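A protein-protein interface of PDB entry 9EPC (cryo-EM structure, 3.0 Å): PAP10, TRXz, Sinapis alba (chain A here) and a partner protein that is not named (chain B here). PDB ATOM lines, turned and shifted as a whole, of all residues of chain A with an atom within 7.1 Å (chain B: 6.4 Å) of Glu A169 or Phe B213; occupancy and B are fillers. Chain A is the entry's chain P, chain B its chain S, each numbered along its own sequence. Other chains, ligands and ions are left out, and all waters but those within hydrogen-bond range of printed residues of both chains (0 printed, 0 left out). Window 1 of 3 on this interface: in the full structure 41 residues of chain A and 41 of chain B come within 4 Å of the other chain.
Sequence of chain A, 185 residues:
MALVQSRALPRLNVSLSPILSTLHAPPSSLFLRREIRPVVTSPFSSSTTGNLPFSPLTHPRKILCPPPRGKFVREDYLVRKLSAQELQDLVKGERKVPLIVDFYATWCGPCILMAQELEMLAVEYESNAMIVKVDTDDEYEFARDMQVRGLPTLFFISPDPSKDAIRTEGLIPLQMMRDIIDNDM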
ATOM      1  N   CYS A 108      19.748  -3.766   3.727  1.00  0.00           N
ATOM      2  CA  CYS A 108      19.889  -4.872   4.662  1.00  0.00           C
ATOM      3  C   CYS A 108      18.551  -5.578   4.831  1.00  0.00           C
ATOM      4  O   CYS A 108      17.559  -4.957   5.225  1.00  0.00           O
ATOM      5  CB  CYS A 108      20.409  -4.357   6.000  1.00  0.00           C
ATOM      6  SG  CYS A 108      20.011  -5.385   7.415  1.00  0.00           S
ATOM      7  N   PRO A 110      17.661  -8.329   6.957  1.00  0.00           N
ATOM      8  CA  PRO A 110      17.225  -8.491   8.352  1.00  0.00           C
ATOM      9  C   PRO A 110      16.821  -7.193   9.026  1.00  0.00           C
ATOM     10  O   PRO A 110      16.007  -7.221   9.956  1.00  0.00           O
ATOM     11  CB  PRO A 110      18.453  -9.115   9.025  1.00  0.00           C
ATOM     12  CG  PRO A 110      19.136  -9.843   7.934  1.00  0.00           C
ATOM     13  CD  PRO A 110      18.948  -9.000   6.709  1.00  0.00           C
ATOM     14  N   GLN A 147      31.149   2.259  16.715  1.00  0.00           N
ATOM     15  CA  GLN A 147      31.650   0.891  16.598  1.00  0.00           C
ATOM     16  C   GLN A 147      30.534  -0.075  16.210  1.00  0.00           C
ATOM     17  O   GLN A 147      30.439  -1.188  16.730  1.00  0.00           O
ATOM     18  CB  GLN A 147      32.346   0.442  17.884  1.00  0.00           C
ATOM     19  CG  GLN A 147      33.577   1.263  18.214  1.00  0.00           C
ATOM     20  CD  GLN A 147      34.416   0.643  19.305  1.00  0.00           C
ATOM     21  OE1 GLN A 147      33.956  -0.234  20.036  1.00  0.00           O
ATOM     22  NE2 GLN A 147      35.661   1.090  19.422  1.00  0.00           N
ATOM     23  N   VAL A 148      29.680   0.361  15.286  1.00  0.00           N
ATOM     24  CA  VAL A 148      28.659  -0.504  14.710  1.00  0.00           C
ATOM     25  C   VAL A 148      29.345  -1.478  13.764  1.00  0.00           C
ATOM     26  O   VAL A 148      29.737  -1.111  12.651  1.00  0.00           O
ATOM     27  CB  VAL A 148      27.577   0.308  13.981  1.00  0.00           C
ATOM     28  CG1 VAL A 148      26.575  -0.619  13.327  1.00  0.00           C
ATOM     29  CG2 VAL A 148      26.885   1.245  14.947  1.00  0.00           C
ATOM     30  N   ARG A 149      29.493  -2.725  14.198  1.00  0.00           N
ATOM     31  CA  ARG A 149      30.246  -3.724  13.458  1.00  0.00           C
ATOM     32  C   ARG A 149      29.417  -4.420  12.390  1.00  0.00           C
ATOM     33  O   ARG A 149      29.937  -5.305  11.703  1.00  0.00           O
ATOM     34  CB  ARG A 149      30.824  -4.759  14.425  1.00  0.00           C
ATOM     35  CG  ARG A 149      31.603  -4.142  15.572  1.00  0.00           C
ATOM     36  CD  ARG A 149      32.222  -5.202  16.459  1.00  0.00           C
ATOM     37  NE  ARG A 149      31.225  -6.111  17.010  1.00  0.00           N
ATOM     38  CZ  ARG A 149      31.508  -7.144  17.790  1.00  0.00           C
ATOM     39  NH1 ARG A 149      32.754  -7.433  18.128  1.00  0.00           N
ATOM     40  NH2 ARG A 149      30.518  -7.907  18.242  1.00  0.00           N
ATOM     41  N   GLY A 150      28.153  -4.053  12.236  1.00  0.00           N
ATOM     42  CA  GLY A 150      27.318  -4.662  11.225  1.00  0.00           C
ATOM     43  C   GLY A 150      25.864  -4.315  11.465  1.00  0.00           C
ATOM     44  O   GLY A 150      25.535  -3.506  12.333  1.00  0.00           O
ATOM     45  N   LEU A 151      25.001  -4.946  10.680  1.00  0.00           N
ATOM     46  CA  LEU A 151      23.584  -4.637  10.717  1.00  0.00           C
ATOM     47  C   LEU A 151      22.766  -5.912  10.830  1.00  0.00           C
ATOM     48  O   LEU A 151      23.176  -6.964  10.332  1.00  0.00           O
ATOM     49  CB  LEU A 151      23.166  -3.869   9.457  1.00  0.00           C
ATOM     50  CG  LEU A 151      24.007  -2.629   9.163  1.00  0.00           C
ATOM     51  CD1 LEU A 151      23.680  -2.085   7.793  1.00  0.00           C
ATOM     52  CD2 LEU A 151      23.785  -1.575  10.229  1.00  0.00           C
ATOM     53  N   PRO A 152      21.601  -5.851  11.487  1.00  0.00           N
ATOM     54  CA  PRO A 152      21.033  -4.707  12.211  1.00  0.00           C
ATOM     55  C   PRO A 152      21.662  -4.543  13.588  1.00  0.00           C
ATOM     56  O   PRO A 152      21.968  -5.525  14.254  1.00  0.00           O
ATOM     57  CB  PRO A 152      19.548  -5.067  12.295  1.00  0.00           C
ATOM     58  CG  PRO A 152      19.553  -6.560  12.393  1.00  0.00           C
ATOM     59  CD  PRO A 152      20.693  -7.011  11.511  1.00  0.00           C
ATOM     60  N   THR A 153      21.864  -3.311  14.042  1.00  0.00           N
ATOM     61  CA  THR A 153      22.459  -3.043  15.342  1.00  0.00           C
ATOM     62  C   THR A 153      21.547  -2.110  16.117  1.00  0.00           C
ATOM     63  O   THR A 153      21.104  -1.088  15.584  1.00  0.00           O
ATOM     64  CB  THR A 153      23.852  -2.425  15.200  1.00  0.00           C
ATOM     65  OG1 THR A 153      24.703  -3.319  14.475  1.00  0.00           O
ATOM     66  CG2 THR A 153      24.457  -2.161  16.566  1.00  0.00           C
ATOM     67  N   LEU A 154      21.264  -2.461  17.367  1.00  0.00           N
ATOM     68  CA  LEU A 154      20.422  -1.655  18.236  1.00  0.00           C
ATOM     69  C   LEU A 154      21.240  -1.131  19.404  1.00  0.00           C
ATOM     70  O   LEU A 154      22.021  -1.871  20.010  1.00  0.00           O
ATOM     71  CB  LEU A 154      19.234  -2.456  18.763  1.00  0.00           C
ATOM     72  CG  LEU A 154      18.217  -2.934  17.733  1.00  0.00           C
ATOM     73  CD1 LEU A 154      17.049  -3.591  18.434  1.00  0.00           C
ATOM     74  CD2 LEU A 154      17.749  -1.775  16.880  1.00  0.00           C
ATOM     75  N   ARG A 167      24.525  -2.485  23.483  1.00  0.00           N
ATOM     76  CA  ARG A 167      24.575  -2.661  22.038  1.00  0.00           C
ATOM     77  C   ARG A 167      24.258  -4.113  21.715  1.00  0.00           C
ATOM     78  O   ARG A 167      24.932  -5.023  22.211  1.00  0.00           O
ATOM     79  CB  ARG A 167      25.943  -2.277  21.479  1.00  0.00           C
ATOM     80  CG  ARG A 167      26.046  -2.426  19.973  1.00  0.00           C
ATOM     81  CD  ARG A 167      27.475  -2.284  19.491  1.00  0.00           C
ATOM     82  NE  ARG A 167      28.315  -3.377  19.960  1.00  0.00           N
ATOM     83  CZ  ARG A 167      29.580  -3.556  19.602  1.00  0.00           C
ATOM     84  NH1 ARG A 167      30.185  -2.729  18.767  1.00  0.00           N
ATOM     85  NH2 ARG A 167      30.252  -4.592  20.094  1.00  0.00           N
ATOM     86  N   THR A 168      23.240  -4.327  20.889  1.00  0.00           N
ATOM     87  CA  THR A 168      22.821  -5.661  20.484  1.00  0.00           C
ATOM     88  C   THR A 168      23.013  -5.808  18.985  1.00  0.00           C
ATOM     89  O   THR A 168      22.541  -4.972  18.209  1.00  0.00           O
ATOM     90  CB  THR A 168      21.363  -5.926  20.854  1.00  0.00           C
ATOM     91  OG1 THR A 168      20.533  -4.922  20.263  1.00  0.00           O
ATOM     92  CG2 THR A 168      21.187  -5.898  22.361  1.00  0.00           C
ATOM     93  N   GLU A 169      23.704  -6.869  18.584  1.00  0.00           N
ATOM     94  CA  GLU A 169      24.003  -7.129  17.185  1.00  0.00           C
ATOM     95  C   GLU A 169      23.297  -8.401  16.747  1.00  0.00           C
ATOM     96  O   GLU A 169      23.348  -9.419  17.445  1.00  0.00           O
ATOM     97  CB  GLU A 169      25.512  -7.241  16.966  1.00  0.00           C
ATOM     98  CG  GLU A 169      26.266  -6.004  17.422  1.00  0.00           C
ATOM     99  CD  GLU A 169      27.683  -5.945  16.895  1.00  0.00           C
ATOM    100  OE1 GLU A 169      28.439  -6.918  17.092  1.00  0.00           O
ATOM    101  OE2 GLU A 169      28.039  -4.922  16.275  1.00  0.00           O
ATOM    102  N   GLY A 170      22.643  -8.339  15.596  1.00  0.00           N
ATOM    103  CA  GLY A 170      21.837  -9.437  15.108  1.00  0.00           C
ATOM    104  C   GLY A 170      20.356  -9.184  15.307  1.00  0.00           C
ATOM    105  O   GLY A 170      19.929  -8.286  16.038  1.00  0.00           O
ATOM    106  N   LEU A 171      19.557 -10.002  14.634  1.00  0.00           N
ATOM    107  CA  LEU A 171      18.103  -9.884  14.686  1.00  0.00           C
ATOM    108  C   LEU A 171      17.635 -10.429  16.029  1.00  0.00           C
ATOM    109  O   LEU A 171      17.283 -11.599  16.165  1.00  0.00           O
ATOM    110  CB  LEU A 171      17.470 -10.623  13.517  1.00  0.00           C
ATOM    111  CG  LEU A 171      16.005 -10.332  13.212  1.00  0.00           C
ATOM    112  CD1 LEU A 171      15.706  -8.871  13.460  1.00  0.00           C
ATOM    113  CD2 LEU A 171      15.716 -10.687  11.774  1.00  0.00           C
ATOM    114  N   ILE A 172      17.642  -9.562  17.037  1.00  0.00           N
ATOM    115  CA  ILE A 172      17.305  -9.937  18.407  1.00  0.00           C
ATOM    116  C   ILE A 172      15.798 -10.157  18.509  1.00  0.00           C
ATOM    117  O   ILE A 172      15.030  -9.535  17.761  1.00  0.00           O
ATOM    118  CB  ILE A 172      17.800  -8.870  19.401  1.00  0.00           C
ATOM    119  CG1 ILE A 172      18.511  -9.522  20.585  1.00  0.00           C
ATOM    120  CG2 ILE A 172      16.662  -8.006  19.894  1.00  0.00           C
ATOM    121  CD1 ILE A 172      19.695 -10.366  20.190  1.00  0.00           C
ATOM    122  N   GLN B 210      26.051 -14.973  15.427  1.00  0.00           N
ATOM    123  CA  GLN B 210      24.969 -14.006  15.325  1.00  0.00           C
ATOM    124  C   GLN B 210      23.770 -14.618  14.608  1.00  0.00           C
ATOM    125  O   GLN B 210      23.911 -15.492  13.750  1.00  0.00           O
ATOM    126  CB  GLN B 210      25.444 -12.763  14.578  1.00  0.00           C
ATOM    127  CG  GLN B 210      26.887 -12.375  14.848  1.00  0.00           C
ATOM    128  CD  GLN B 210      27.069 -11.641  16.161  1.00  0.00           C
ATOM    129  OE1 GLN B 210      26.140 -11.531  16.960  1.00  0.00           O
ATOM    130  NE2 GLN B 210      28.273 -11.130  16.388  1.00  0.00           N
ATOM    131  N   HIS B 211      22.576 -14.150  14.971  1.00  0.00           N
ATOM    132  CA  HIS B 211      21.354 -14.742  14.433  1.00  0.00           C
ATOM    133  C   HIS B 211      21.173 -14.395  12.960  1.00  0.00           C
ATOM    134  O   HIS B 211      21.199 -15.275  12.093  1.00  0.00           O
ATOM    135  CB  HIS B 211      20.147 -14.272  15.245  1.00  0.00           C
ATOM    136  CG  HIS B 211      18.832 -14.672  14.656  1.00  0.00           C
ATOM    137  ND1 HIS B 211      17.712 -13.873  14.728  1.00  0.00           N
ATOM    138  CD2 HIS B 211      18.455 -15.788  13.990  1.00  0.00           C
ATOM    139  CE1 HIS B 211      16.703 -14.477  14.127  1.00  0.00           C
ATOM    140  NE2 HIS B 211      17.127 -15.641  13.670  1.00  0.00           N
ATOM    141  N   ALA B 212      20.990 -13.113  12.658  1.00  0.00           N
ATOM    142  CA  ALA B 212      20.836 -12.630  11.284  1.00  0.00           C
ATOM    143  C   ALA B 212      21.546 -11.281  11.239  1.00  0.00           C
ATOM    144  O   ALA B 212      20.954 -10.245  11.547  1.00  0.00           O
ATOM    145  CB  ALA B 212      19.373 -12.520  10.880  1.00  0.00           C
ATOM    146  N   PHE B 213      22.815 -11.304  10.851  1.00  0.00           N
ATOM    147  CA  PHE B 213      23.693 -10.159  11.066  1.00  0.00           C
ATOM    148  C   PHE B 213      24.699 -10.110   9.928  1.00  0.00           C
ATOM    149  O   PHE B 213      25.549 -10.997   9.813  1.00  0.00           O
ATOM    150  CB  PHE B 213      24.378 -10.282  12.421  1.00  0.00           C
ATOM    151  CG  PHE B 213      25.458  -9.278  12.662  1.00  0.00           C
ATOM    152  CD1 PHE B 213      25.157  -8.025  13.158  1.00  0.00           C
ATOM    153  CD2 PHE B 213      26.782  -9.605  12.434  1.00  0.00           C
ATOM    154  CE1 PHE B 213      26.154  -7.109  13.399  1.00  0.00           C
ATOM    155  CE2 PHE B 213      27.782  -8.693  12.670  1.00  0.00           C
ATOM    156  CZ  PHE B 213      27.469  -7.446  13.155  1.00  0.00           C
ATOM    157  N   VAL B 214      24.601  -9.079   9.096  1.00  0.00           N
ATOM    158  CA  VAL B 214      25.481  -8.929   7.942  1.00  0.00           C
ATOM    159  C   VAL B 214      26.636  -8.007   8.312  1.00  0.00           C
ATOM    160  O   VAL B 214      26.429  -6.998   9.000  1.00  0.00           O
ATOM    161  CB  VAL B 214      24.712  -8.403   6.722  1.00  0.00           C
ATOM    162  CG1 VAL B 214      23.732  -9.445   6.241  1.00  0.00           C
ATOM    163  CG2 VAL B 214      23.980  -7.120   7.066  1.00  0.00           C
ATOM    164  N   PRO B 215      27.865  -8.322   7.900  1.00  0.00           N
ATOM    165  CA  PRO B 215      28.982  -7.420   8.218  1.00  0.00           C
ATOM    166  C   PRO B 215      28.840  -6.057   7.568  1.00  0.00           C
ATOM    167  O   PRO B 215      28.878  -5.031   8.259  1.00  0.00           O
ATOM    168  CB  PRO B 215      30.205  -8.186   7.694  1.00  0.00           C
ATOM    169  CG  PRO B 215      29.760  -9.606   7.595  1.00  0.00           C
ATOM    170  CD  PRO B 215      28.319  -9.545   7.224  1.00  0.00           C
ATOM    171  N   GLY B 247      28.356 -11.904   3.106  1.00  0.00           N
ATOM    172  CA  GLY B 247      27.922 -13.134   3.727  1.00  0.00           C
ATOM    173  C   GLY B 247      27.372 -12.851   5.113  1.00  0.00           C
ATOM    174  O   GLY B 247      26.881 -11.757   5.382  1.00  0.00           O
ATOM    175  N   GLY B 248      27.469 -13.854   5.977  1.00  0.00           N
ATOM    176  CA  GLY B 248      26.996 -13.759   7.338  1.00  0.00           C
ATOM    177  C   GLY B 248      28.101 -14.087   8.325  1.00  0.00           C
ATOM    178  O   GLY B 248      29.290 -13.957   8.033  1.00  0.00           O
ATOM    179  N   CYS B 249      27.684 -14.523   9.509  1.00  0.00           N
ATOM    180  CA  CYS B 249      28.629 -14.873  10.553  1.00  0.00           C
ATOM    181  C   CYS B 249      29.251 -16.239  10.273  1.00  0.00           C
ATOM    182  O   CYS B 249      28.882 -16.944   9.330  1.00  0.00           O
ATOM    183  CB  CYS B 249      27.943 -14.874  11.917  1.00  0.00           C
ATOM    184  SG  CYS B 249      26.626 -16.098  12.073  1.00  0.00           S
ATOM    185  N   PHE B 275      18.674 -16.389  24.768  1.00  0.00           N
ATOM    186  CA  PHE B 275      19.146 -16.312  23.390  1.00  0.00           C
ATOM    187  C   PHE B 275      20.301 -17.272  23.151  1.00  0.00           C
ATOM    188  O   PHE B 275      20.355 -17.948  22.118  1.00  0.00           O
ATOM    189  CB  PHE B 275      19.559 -14.884  23.058  1.00  0.00           C
ATOM    190  CG  PHE B 275      19.621 -14.599  21.589  1.00  0.00           C
ATOM    191  CD1 PHE B 275      18.501 -14.752  20.794  1.00  0.00           C
ATOM    192  CD2 PHE B 275      20.793 -14.160  21.004  1.00  0.00           C
ATOM    193  CE1 PHE B 275      18.552 -14.486  19.444  1.00  0.00           C
ATOM    194  CE2 PHE B 275      20.850 -13.892  19.655  1.00  0.00           C
ATOM    195  CZ  PHE B 275      19.728 -14.055  18.875  1.00  0.00           C
ATOM    196  N   ALA B 302      25.111 -11.354  22.706  1.00  0.00           N
ATOM    197  CA  ALA B 302      24.830 -10.242  21.795  1.00  0.00           C
ATOM    198  C   ALA B 302      24.199  -9.056  22.519  1.00  0.00           C
ATOM    199  O   ALA B 302      23.286  -8.410  22.006  1.00  0.00           O
ATOM    200  CB  ALA B 302      23.947 -10.695  20.632  1.00  0.00           C
ATOM    201  N   CYS B 303      24.676  -8.775  23.727  1.00  0.00           N
ATOM    202  CA  CYS B 303      24.194  -7.639  24.506  1.00  0.00           C
ATOM    203  C   CYS B 303      25.362  -6.943  25.192  1.00  0.00           C
ATOM    204  O   CYS B 303      25.315  -6.624  26.381  1.00  0.00           O
ATOM    205  CB  CYS B 303      23.140  -8.077  25.518  1.00  0.00           C
ATOM    206  SG  CYS B 303      21.614  -8.686  24.776  1.00  0.00           S
ATOM    207  N   SER B 304      26.438  -6.711  24.444  1.00  0.00           N
ATOM    208  CA  SER B 304      27.614  -6.066  25.009  1.00  0.00           C
ATOM    209  C   SER B 304      27.276  -4.668  25.514  1.00  0.00           C
ATOM    210  O   SER B 304      26.603  -3.889  24.836  1.00  0.00           O
ATOM    211  CB  SER B 304      28.727  -5.990  23.965  1.00  0.00           C
ATOM    212  OG  SER B 304      28.338  -5.188  22.866  1.00  0.00           O
ATOM    213  N   CYS B 322      30.372  -8.826  24.507  1.00  0.00           N
ATOM    214  CA  CYS B 322      29.241  -9.739  24.482  1.00  0.00           C
ATOM    215  C   CYS B 322      29.727 -11.173  24.682  1.00  0.00           C
ATOM    216  O   CYS B 322      30.925 -11.452  24.770  1.00  0.00           O
ATOM    217  CB  CYS B 322      28.468  -9.597  23.176  1.00  0.00           C
ATOM    218  SG  CYS B 322      29.385 -10.085  21.703  1.00  0.00           S
ATOM    219  N   GLU B 324      29.677 -13.789  22.663  1.00  0.00           N
ATOM    220  CA  GLU B 324      30.522 -14.246  21.563  1.00  0.00           C
ATOM    221  C   GLU B 324      31.582 -13.207  21.215  1.00  0.00           C
ATOM    222  O   GLU B 324      31.816 -12.874  20.056  1.00  0.00           O
ATOM    223  CB  GLU B 324      29.663 -14.582  20.350  1.00  0.00           C
ATOM    224  CG  GLU B 324      28.679 -13.495  19.952  1.00  0.00           C
ATOM    225  CD  GLU B 324      27.374 -13.570  20.718  1.00  0.00           C
ATOM    226  OE1 GLU B 324      27.298 -14.346  21.693  1.00  0.00           O
ATOM    227  OE2 GLU B 324      26.421 -12.855  20.345  1.00  0.00           O
ATOM    228  N   ASP B 325      32.238 -12.698  22.254  1.00  0.00           N
ATOM    229  CA  ASP B 325      33.460 -11.924  22.112  1.00  0.00           C
ATOM    230  C   ASP B 325      34.426 -12.168  23.257  1.00  0.00           C
ATOM    231  O   ASP B 325      35.496 -11.552  23.281  1.00  0.00           O
ATOM    232  CB  ASP B 325      33.149 -10.423  22.017  1.00  0.00           C
ATOM    233  CG  ASP B 325      32.839  -9.978  20.602  1.00  0.00           C
ATOM    234  OD1 ASP B 325      33.377 -10.589  19.656  1.00  0.00           O
ATOM    235  OD2 ASP B 325      32.066  -9.012  20.437  1.00  0.00           O
ATOM    236  N   HIS B 348      35.305 -10.677  11.342  1.00  0.00           N
ATOM    237  CA  HIS B 348      34.552 -10.226  12.504  1.00  0.00           C
ATOM    238  C   HIS B 348      35.173 -10.701  13.810  1.00  0.00           C
ATOM    239  O   HIS B 348      34.914 -10.105  14.861  1.00  0.00           O
ATOM    240  CB  HIS B 348      33.105 -10.705  12.413  1.00  0.00           C
ATOM    241  CG  HIS B 348      32.223 -10.160  13.491  1.00  0.00           C
ATOM    242  ND1 HIS B 348      32.076 -10.777  14.714  1.00  0.00           N
ATOM    243  CD2 HIS B 348      31.449  -9.051  13.533  1.00  0.00           C
ATOM    244  CE1 HIS B 348      31.244 -10.074  15.461  1.00  0.00           C
ATOM    245  NE2 HIS B 348      30.849  -9.022  14.768  1.00  0.00           N
ATOM    246  N   SER B 488      22.973 -12.244   1.685  1.00  0.00           N
ATOM    247  CA  SER B 488      23.913 -12.852   2.618  1.00  0.00           C
ATOM    248  C   SER B 488      23.873 -14.371   2.548  1.00  0.00           C
ATOM    249  O   SER B 488      24.894 -15.026   2.782  1.00  0.00           O
ATOM    250  CB  SER B 488      23.619 -12.379   4.039  1.00  0.00           C
ATOM    251  OG  SER B 488      22.275 -12.647   4.391  1.00  0.00           O
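O of Pro A152 sits at hydrogen-bond distance from N of Gly A170, at 3.2 Å. O of Leu A154 sits at hydrogen-bond distance from N of Thr A168 (2.9 Å). NH1 of Arg A167 is in salt-bridge range of OE2 of Glu A169, at 3.95 Å. O of Gln B210 lies within hydrogen-bond range of SG of Cys B249 (3.2 Å). The backbone NH (N) of Ala B302 lies within hydrogen-bond range of the side-chain carboxylate (OE2) of Glu B324 (3.1 Å). The side-chain sulfur (SG) of Cys B322 sits at hydrogen-bond distance from the side-chain carboxylate (OD2) of Asp B325 (3.2 Å).
OD2 of Asp B325 lies within salt-bridge range of NH1 of Arg A149, at 2.9 Å. The backbone carbonyl oxygen (O) of Leu A151 sits at hydrogen-bond distance from the backbone NH (N) of Val B214 (2.8 Å). The backbone NH (N) of Arg A167 sits at hydrogen-bond distance from the backbone carbonyl oxygen (O) of Ser B304. The backbone carbonyl oxygen of Leu A171 is in hydrogen-bond range of a ring nitrogen (ND1) of His B211. O of Ala B212 is in hydrogen-bond range of N of Leu A171 (3.4 Å).
Of chain B, only Gln B210 (3.5 Å), Phe B213 (3.6 Å), Ala B302 (3.5 Å) and His B348 (3.95 Å) come within 4 Å of Glu A169. Of chain A, only Arg A149, Gly A150, Leu A151, Glu A169 and Gly A170 come within 4 Å of Phe B213. Printed residues of chain B within 4 Å of Ile A172: Phe B275. Of the printed residues of chain B, Arg A167 touches Ala B302 (3.8 Å), Cys B303 (3.6 Å) and Ser B304 (2.8 Å). Printed residues of chain A within 4 Å of Asp B325: Arg A149. Printed residues of chain A within 4 Å of Ala B212: Pro A110 (3.7 Å), Pro A152 (3.2 Å), Gly A170 (3.8 Å) and Leu A171 (3.4 Å). Of the printed residues of chain A, His B348 touches Arg A149 (3.6 Å) and Glu A169 (3.95 Å). Glu B324 touches none of the printed residues of chain A. Cys B249 touches none of the printed residues of chain A. The nearest printed residue of chain A that does not touch Phe B213 is Pro A152 (4.2 Å).
Hydrophobic or aromatic side chains of chain B that line the printed part of chain A: His B211, Ala B212, Phe B213, Val B214, Phe B275, Ala B302 and His B348. Along chain B the printed residues that touch a printed residue of chain A span positions 210 to 348. Among the printed residues, 25 pairs touch across the chains.
O of Ala B212 touches CB of Pro A110 (3.7 Å). Phe B213 touches Arg A149 (CZ to O, 3.6 Å). CZ of Phe B213 touches CA of Gly A150, 3.4 Å away. Pro B215 touches Gly A150 (O to CA, 3.4 Å). O of Leu A151 touches CA of Phe B213 (3.3 Å). O of Arg A167 touches O of Ala B302 (3.8 Å). Thr A168 touches Cys B303. Glu A169 touches Phe B213. Glu A169 touches Ala B302 (O to CB, 3.5 Å). Gly A170 touches Phe B213.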
